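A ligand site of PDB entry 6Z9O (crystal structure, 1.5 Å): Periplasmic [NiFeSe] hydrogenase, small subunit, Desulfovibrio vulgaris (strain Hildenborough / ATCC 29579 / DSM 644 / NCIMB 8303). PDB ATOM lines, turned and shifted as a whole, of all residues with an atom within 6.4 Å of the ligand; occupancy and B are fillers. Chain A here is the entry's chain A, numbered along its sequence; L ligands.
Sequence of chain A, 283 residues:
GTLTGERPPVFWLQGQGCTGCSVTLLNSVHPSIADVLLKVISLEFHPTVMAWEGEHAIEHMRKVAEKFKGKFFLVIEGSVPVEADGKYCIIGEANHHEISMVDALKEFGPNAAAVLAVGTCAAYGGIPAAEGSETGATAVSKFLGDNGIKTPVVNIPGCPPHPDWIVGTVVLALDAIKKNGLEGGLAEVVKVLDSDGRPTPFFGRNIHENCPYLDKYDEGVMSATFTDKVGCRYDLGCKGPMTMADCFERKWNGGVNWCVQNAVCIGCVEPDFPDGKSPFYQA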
ATOM      1  N   ILE A 207      -9.578   7.898  14.148  1.00  0.00           N
ATOM      2  CA  ILE A 207      -8.524   8.666  13.488  1.00  0.00           C
ATOM      3  C   ILE A 207      -7.685   9.410  14.508  1.00  0.00           C
ATOM      4  O   ILE A 207      -6.449   9.322  14.517  1.00  0.00           O
ATOM      5  CB  ILE A 207      -9.130   9.640  12.455  1.00  0.00           C
ATOM      6  CG1 ILE A 207      -9.726   8.863  11.278  1.00  0.00           C
ATOM      7  CG2 ILE A 207      -8.071  10.664  11.986  1.00  0.00           C
ATOM      8  CD1 ILE A 207     -10.004   9.686  10.060  1.00  0.00           C
ATOM      9  N   HIS A 208      -8.351  10.176  15.374  1.00  0.00           N
ATOM     10  CA  HIS A 208      -7.637  11.075  16.281  1.00  0.00           C
ATOM     11  C   HIS A 208      -6.744  10.305  17.245  1.00  0.00           C
ATOM     12  O   HIS A 208      -5.589  10.689  17.474  1.00  0.00           O
ATOM     13  CB  HIS A 208      -8.686  11.931  17.020  1.00  0.00           C
ATOM     14  CG  HIS A 208      -8.169  12.679  18.210  1.00  0.00           C
ATOM     15  ND1 HIS A 208      -7.561  13.913  18.115  1.00  0.00           N
ATOM     16  CD2 HIS A 208      -8.250  12.404  19.530  1.00  0.00           C
ATOM     17  CE1 HIS A 208      -7.254  14.346  19.319  1.00  0.00           C
ATOM     18  NE2 HIS A 208      -7.664  13.446  20.203  1.00  0.00           N
ATOM     19  N   GLU A 209      -7.242   9.188  17.794  1.00  0.00           N
ATOM     20  CA  GLU A 209      -6.457   8.427  18.759  1.00  0.00           C
ATOM     21  C   GLU A 209      -5.203   7.827  18.137  1.00  0.00           C
ATOM     22  O   GLU A 209      -4.277   7.468  18.881  1.00  0.00           O
ATOM     23  CB  GLU A 209      -7.312   7.329  19.371  1.00  0.00           C
ATOM     24  CG  GLU A 209      -8.473   7.856  20.188  1.00  0.00           C
ATOM     25  CD  GLU A 209      -8.015   8.643  21.400  1.00  0.00           C
ATOM     26  OE1 GLU A 209      -7.126   8.166  22.128  1.00  0.00           O
ATOM     27  OE2 GLU A 209      -8.543   9.752  21.611  1.00  0.00           O
ATOM     28  N   CYS A 211      -3.607   9.519  15.495  1.00  0.00           N
ATOM     29  CA  CYS A 211      -3.157  10.594  14.620  1.00  0.00           C
ATOM     30  C   CYS A 211      -1.708  10.976  14.928  1.00  0.00           C
ATOM     31  O   CYS A 211      -1.333  11.107  16.105  1.00  0.00           O
ATOM     32  CB  CYS A 211      -4.039  11.822  14.773  1.00  0.00           C
ATOM     33  SG  CYS A 211      -3.563  13.190  13.690  1.00  0.00           S
ATOM     34  N   PRO A 212      -0.880  11.203  13.908  1.00  0.00           N
ATOM     35  CA  PRO A 212       0.503  11.636  14.172  1.00  0.00           C
ATOM     36  C   PRO A 212       0.614  12.978  14.857  1.00  0.00           C
ATOM     37  O   PRO A 212       1.669  13.272  15.434  1.00  0.00           O
ATOM     38  CB  PRO A 212       1.128  11.682  12.765  1.00  0.00           C
ATOM     39  CG  PRO A 212      -0.004  11.809  11.837  1.00  0.00           C
ATOM     40  CD  PRO A 212      -1.134  11.050  12.464  1.00  0.00           C
ATOM     41  N   TYR A 213      -0.415  13.820  14.812  1.00  0.00           N
ATOM     42  CA  TYR A 213      -0.353  15.124  15.465  1.00  0.00           C
ATOM     43  C   TYR A 213      -1.002  15.114  16.845  1.00  0.00           C
ATOM     44  O   TYR A 213      -1.235  16.186  17.423  1.00  0.00           O
ATOM     45  CB  TYR A 213      -0.986  16.184  14.571  1.00  0.00           C
ATOM     46  CG  TYR A 213      -0.480  16.090  13.141  1.00  0.00           C
ATOM     47  CD1 TYR A 213       0.828  16.445  12.811  1.00  0.00           C
ATOM     48  CD2 TYR A 213      -1.308  15.624  12.129  1.00  0.00           C
ATOM     49  CE1 TYR A 213       1.289  16.351  11.496  1.00  0.00           C
ATOM     50  CE2 TYR A 213      -0.855  15.525  10.819  1.00  0.00           C
ATOM     51  CZ  TYR A 213       0.440  15.879  10.510  1.00  0.00           C
ATOM     52  OH  TYR A 213       0.848  15.759   9.191  1.00  0.00           O
ATOM     53  N   LEU A 214      -1.279  13.930  17.403  1.00  0.00           N
ATOM     54  CA  LEU A 214      -1.914  13.869  18.717  1.00  0.00           C
ATOM     55  C   LEU A 214      -1.032  14.483  19.799  1.00  0.00           C
ATOM     56  O   LEU A 214      -1.545  15.051  20.765  1.00  0.00           O
ATOM     57  CB  LEU A 214      -2.244  12.400  19.065  1.00  0.00           C
ATOM     58  CG  LEU A 214      -3.113  12.137  20.303  1.00  0.00           C
ATOM     59  CD1 LEU A 214      -4.517  12.729  20.162  1.00  0.00           C
ATOM     60  CD2 LEU A 214      -3.212  10.640  20.562  1.00  0.00           C
ATOM     61  N   ASP A 215       0.295  14.417  19.640  1.00  0.00           N
ATOM     62  CA  ASP A 215       1.168  15.053  20.620  1.00  0.00           C
ATOM     63  C   ASP A 215       0.945  16.559  20.643  1.00  0.00           C
ATOM     64  O   ASP A 215       0.939  17.170  21.720  1.00  0.00           O
ATOM     65  CB  ASP A 215       2.631  14.701  20.328  1.00  0.00           C
ATOM     66  CG  ASP A 215       3.111  15.186  18.960  1.00  0.00           C
ATOM     67  OD1 ASP A 215       2.309  15.239  18.004  1.00  0.00           O
ATOM     68  OD2 ASP A 215       4.324  15.509  18.849  1.00  0.00           O
ATOM     69  N   LYS A 216       0.747  17.167  19.475  1.00  0.00           N
ATOM     70  CA  LYS A 216       0.468  18.602  19.428  1.00  0.00           C
ATOM     71  C   LYS A 216      -0.906  18.909  20.018  1.00  0.00           C
ATOM     72  O   LYS A 216      -1.079  19.918  20.704  1.00  0.00           O
ATOM     73  CB  LYS A 216       0.557  19.111  17.988  1.00  0.00           C
ATOM     74  CG  LYS A 216       1.916  18.894  17.348  1.00  0.00           C
ATOM     75  CD  LYS A 216       3.025  19.609  18.130  1.00  0.00           C
ATOM     76  CE  LYS A 216       4.387  19.350  17.518  1.00  0.00           C
ATOM     77  NZ  LYS A 216       5.459  19.791  18.445  1.00  0.00           N
ATOM     78  N   TYR A 217      -1.890  18.040  19.751  1.00  0.00           N
ATOM     79  CA  TYR A 217      -3.194  18.189  20.381  1.00  0.00           C
ATOM     80  C   TYR A 217      -3.062  18.198  21.900  1.00  0.00           C
ATOM     81  O   TYR A 217      -3.579  19.091  22.573  1.00  0.00           O
ATOM     82  CB  TYR A 217      -4.120  17.071  19.929  1.00  0.00           C
ATOM     83  CG  TYR A 217      -5.484  17.107  20.572  1.00  0.00           C
ATOM     84  CD1 TYR A 217      -6.534  17.804  19.984  1.00  0.00           C
ATOM     85  CD2 TYR A 217      -5.728  16.438  21.765  1.00  0.00           C
ATOM     86  CE1 TYR A 217      -7.782  17.835  20.560  1.00  0.00           C
ATOM     87  CE2 TYR A 217      -6.978  16.464  22.353  1.00  0.00           C
ATOM     88  CZ  TYR A 217      -8.002  17.164  21.748  1.00  0.00           C
ATOM     89  OH  TYR A 217      -9.242  17.200  22.319  1.00  0.00           O
ATOM     90  N   MET A 222      -1.779  24.407  18.304  1.00  0.00           N
ATOM     91  CA  MET A 222      -2.785  24.389  17.245  1.00  0.00           C
ATOM     92  C   MET A 222      -2.349  25.262  16.083  1.00  0.00           C
ATOM     93  O   MET A 222      -1.901  26.394  16.290  1.00  0.00           O
ATOM     94  CB  MET A 222      -4.141  24.891  17.740  1.00  0.00           C
ATOM     95  CG  MET A 222      -4.762  24.079  18.842  1.00  0.00           C
ATOM     96  SD  MET A 222      -5.170  22.427  18.266  1.00  0.00           S
ATOM     97  CE  MET A 222      -5.550  21.639  19.828  1.00  0.00           C
ATOM     98  N   GLY A 231       1.353  22.278  13.821  1.00  0.00           N
ATOM     99  CA  GLY A 231       0.334  22.167  14.842  1.00  0.00           C
ATOM    100  C   GLY A 231      -0.724  21.131  14.540  1.00  0.00           C
ATOM    101  O   GLY A 231      -0.833  20.591  13.442  1.00  0.00           O
ATOM    102  N   CYS A 232      -1.512  20.845  15.574  1.00  0.00           N
ATOM    103  CA  CYS A 232      -2.741  20.085  15.403  1.00  0.00           C
ATOM    104  C   CYS A 232      -3.764  20.928  14.647  1.00  0.00           C
ATOM    105  O   CYS A 232      -3.766  22.152  14.723  1.00  0.00           O
ATOM    106  CB  CYS A 232      -3.278  19.660  16.770  1.00  0.00           C
ATOM    107  SG  CYS A 232      -4.979  19.080  16.825  1.00  0.00           S
ATOM    108  N   ARG A 233      -4.632  20.233  13.899  1.00  0.00           N
ATOM    109  CA  ARG A 233      -5.620  20.835  13.012  1.00  0.00           C
ATOM    110  C   ARG A 233      -6.984  21.055  13.669  1.00  0.00           C
ATOM    111  O   ARG A 233      -7.944  21.409  12.972  1.00  0.00           O
ATOM    112  CB  ARG A 233      -5.811  19.952  11.775  1.00  0.00           C
ATOM    113  CG  ARG A 233      -4.700  19.994  10.719  1.00  0.00           C
ATOM    114  CD  ARG A 233      -3.356  19.437  11.174  1.00  0.00           C
ATOM    115  NE  ARG A 233      -2.561  19.039  10.015  1.00  0.00           N
ATOM    116  CZ  ARG A 233      -1.225  18.968   9.971  1.00  0.00           C
ATOM    117  NH1 ARG A 233      -0.498  19.264  11.028  1.00  0.00           N
ATOM    118  NH2 ARG A 233      -0.625  18.593   8.852  1.00  0.00           N
ATOM    119  N   TYR A 234      -7.092  20.873  14.984  1.00  0.00           N
ATOM    120  CA  TYR A 234      -8.408  20.891  15.628  1.00  0.00           C
ATOM    121  C   TYR A 234      -9.075  22.257  15.495  1.00  0.00           C
ATOM    122  O   TYR A 234     -10.271  22.339  15.164  1.00  0.00           O
ATOM    123  CB  TYR A 234      -8.251  20.515  17.101  1.00  0.00           C
ATOM    124  CG  TYR A 234      -9.541  20.494  17.880  1.00  0.00           C
ATOM    125  CD1 TYR A 234     -10.339  19.359  17.899  1.00  0.00           C
ATOM    126  CD2 TYR A 234      -9.956  21.598  18.611  1.00  0.00           C
ATOM    127  CE1 TYR A 234     -11.517  19.336  18.627  1.00  0.00           C
ATOM    128  CE2 TYR A 234     -11.130  21.587  19.337  1.00  0.00           C
ATOM    129  CZ  TYR A 234     -11.909  20.452  19.343  1.00  0.00           C
ATOM    130  OH  TYR A 234     -13.075  20.446  20.064  1.00  0.00           O
ATOM    131  N   ASP A 235      -8.345  23.335  15.759  1.00  0.00           N
ATOM    132  CA  ASP A 235      -8.956  24.655  15.678  1.00  0.00           C
ATOM    133  C   ASP A 235      -9.362  25.009  14.262  1.00  0.00           C
ATOM    134  O   ASP A 235     -10.248  25.850  14.071  1.00  0.00           O
ATOM    135  CB  ASP A 235      -8.011  25.731  16.233  1.00  0.00           C
ATOM    136  CG  ASP A 235      -7.944  25.729  17.759  1.00  0.00           C
ATOM    137  OD1 ASP A 235      -8.752  25.008  18.379  1.00  0.00           O
ATOM    138  OD2 ASP A 235      -7.101  26.450  18.321  1.00  0.00           O
ATOM    139  N   CYS A 238     -10.782  20.142  12.328  1.00  0.00           N
ATOM    140  CA  CYS A 238     -10.562  18.703  12.147  1.00  0.00           C
ATOM    141  C   CYS A 238     -11.563  17.886  12.958  1.00  0.00           C
ATOM    142  O   CYS A 238     -11.706  18.085  14.168  1.00  0.00           O
ATOM    143  CB  CYS A 238      -9.147  18.336  12.568  1.00  0.00           C
ATOM    144  SG  CYS A 238      -8.743  16.607  12.244  1.00  0.00           S
ATOM    145  N   LYS A 239     -12.243  16.956  12.292  1.00  0.00           N
ATOM    146  CA  LYS A 239     -13.250  16.096  12.906  1.00  0.00           C
ATOM    147  C   LYS A 239     -12.713  14.702  13.222  1.00  0.00           C
ATOM    148  O   LYS A 239     -13.503  13.785  13.509  1.00  0.00           O
ATOM    149  CB  LYS A 239     -14.487  15.993  12.005  1.00  0.00           C
ATOM    150  CG  LYS A 239     -15.106  17.346  11.667  1.00  0.00           C
ATOM    151  CD  LYS A 239     -15.517  18.085  12.929  1.00  0.00           C
ATOM    152  CE  LYS A 239     -16.371  19.306  12.659  1.00  0.00           C
ATOM    153  NZ  LYS A 239     -15.637  20.319  11.899  1.00  0.00           N
ATOM    154  N   GLY A 240     -11.390  14.515  13.183  1.00  0.00           N
ATOM    155  CA  GLY A 240     -10.790  13.246  13.545  1.00  0.00           C
ATOM    156  C   GLY A 240     -11.246  12.656  14.858  1.00  0.00           C
ATOM    157  O   GLY A 240     -11.359  11.428  14.970  1.00  0.00           O
ATOM    158  N   PRO A 241     -11.500  13.477  15.902  1.00  0.00           N
ATOM    159  CA  PRO A 241     -11.966  12.908  17.176  1.00  0.00           C
ATOM    160  C   PRO A 241     -13.223  12.074  17.063  1.00  0.00           C
ATOM    161  O   PRO A 241     -13.386  11.124  17.845  1.00  0.00           O
ATOM    162  CB  PRO A 241     -12.203  14.151  18.048  1.00  0.00           C
ATOM    163  CG  PRO A 241     -11.229  15.141  17.535  1.00  0.00           C
ATOM    164  CD  PRO A 241     -11.145  14.902  16.044  1.00  0.00           C
ATOM    165  N   TRP A 258      -3.001  12.517   2.842  1.00  0.00           N
ATOM    166  CA  TRP A 258      -4.313  12.275   3.411  1.00  0.00           C
ATOM    167  C   TRP A 258      -4.867  13.577   3.959  1.00  0.00           C
ATOM    168  O   TRP A 258      -4.167  14.586   4.050  1.00  0.00           O
ATOM    169  CB  TRP A 258      -4.288  11.164   4.468  1.00  0.00           C
ATOM    170  CG  TRP A 258      -3.547  11.439   5.719  1.00  0.00           C
ATOM    171  CD1 TRP A 258      -2.229  11.758   5.840  1.00  0.00           C
ATOM    172  CD2 TRP A 258      -4.061  11.375   7.060  1.00  0.00           C
ATOM    173  NE1 TRP A 258      -1.891  11.913   7.167  1.00  0.00           N
ATOM    174  CE2 TRP A 258      -3.004  11.687   7.931  1.00  0.00           C
ATOM    175  CE3 TRP A 258      -5.317  11.085   7.596  1.00  0.00           C
ATOM    176  CZ2 TRP A 258      -3.164  11.716   9.324  1.00  0.00           C
ATOM    177  CZ3 TRP A 258      -5.475  11.119   8.976  1.00  0.00           C
ATOM    178  CH2 TRP A 258      -4.402  11.423   9.822  1.00  0.00           C
ATOM    179  N   VAL A 260      -5.854  14.891   6.792  1.00  0.00           N
ATOM    180  CA  VAL A 260      -5.362  15.621   7.947  1.00  0.00           C
ATOM    181  C   VAL A 260      -4.016  16.262   7.656  1.00  0.00           C
ATOM    182  O   VAL A 260      -3.741  17.386   8.102  1.00  0.00           O
ATOM    183  CB  VAL A 260      -5.295  14.695   9.173  1.00  0.00           C
ATOM    184  CG1 VAL A 260      -4.619  15.403  10.335  1.00  0.00           C
ATOM    185  CG2 VAL A 260      -6.688  14.211   9.543  1.00  0.00           C
ATOM    186  N   CYS A 265      -9.664  16.580   8.458  1.00  0.00           N
ATOM    187  CA  CYS A 265     -10.646  15.522   8.284  1.00  0.00           C
ATOM    188  C   CYS A 265     -12.041  16.105   8.488  1.00  0.00           C
ATOM    189  O   CYS A 265     -12.255  16.911   9.394  1.00  0.00           O
ATOM    190  CB  CYS A 265     -10.378  14.381   9.269  1.00  0.00           C
ATOM    191  SG  CYS A 265     -11.621  13.079   9.361  1.00  0.00           S
HETATM  192 FE1  LIG L   1      -7.242  16.162  13.924  1.00  0.00          FE
HETATM  193 FE2  LIG L   1      -6.951  14.883  16.373  1.00  0.00          FE
HETATM  194 FE3  LIG L   1      -5.473  17.094  15.834  1.00  0.00          FE
HETATM  195 FE4  LIG L   1      -4.985  14.721  14.534  1.00  0.00          FE
HETATM  196  S1  LIG L   1      -4.693  15.139  16.758  1.00  0.00           S
HETATM  197  S2  LIG L   1      -5.066  16.815  13.592  1.00  0.00           S
HETATM  198  S3  LIG L   1      -7.123  13.914  14.307  1.00  0.00           S
HETATM  199  S4  LIG L   1      -7.762  17.010  15.994  1.00  0.00           S
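N of Leu 214 lies close to S1 of the ligand. SG of Cys 232 binds FE3 of the ligand (2.3 Å). A sulfur (S2) of the ligand sits close to the backbone NH of Arg 233 (3.5 Å). SG of Cys 238 is bound to FE1 of the ligand, 2.3 Å away. An iron atom (FE4) of the ligand is bound by the side-chain sulfur (SG) of Cys 211. ND1 of His 208 binds FE2 of the ligand.
SG of Cys 238 sits close to N of Gly 240 (3.5 Å). SG of Cys 232 lies close to SD of Met 222, 3.6 Å away. The backbone carbonyl oxygen (O) of Arg 233 is in hydrogen-bond range of the backbone NH (N) of Cys 238, at 3.2 Å. N of His 208 is in hydrogen-bond range of O of Gly 240. NH1 of Arg 233 sits at hydrogen-bond distance from O of Gly 231, 2.8 Å away. OH of Tyr 213 lies within hydrogen-bond range of NH2 of Arg 233, 3.2 Å away. NE of Arg 233 is in hydrogen-bond range of O of Val 260 (2.8 Å). The backbone NH (N) of Tyr 213 lies close to the side-chain sulfur (SG) of Cys 211.
S1 of the ligand sits close to O of Tyr 213 (3.7 Å). Residues that only touch the ligand: Val 260, Tyr 234, Tyr 217, Gly 240 and Pro 241. Hydrophobic or aromatic side chains within 4 Å of the ligand: His 208, Tyr 217, Tyr 234, Pro 241 and Val 260. Within 4 Å of the ligand: His 208, Cys 211, Tyr 213, Leu 214, Tyr 217, Cys 232, Arg 233, Tyr 234, Cys 238, Gly 240, Pro 241 and Val 260. The nearest printed residue that does not touch the ligand is Ile 207 (4.1 Å).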
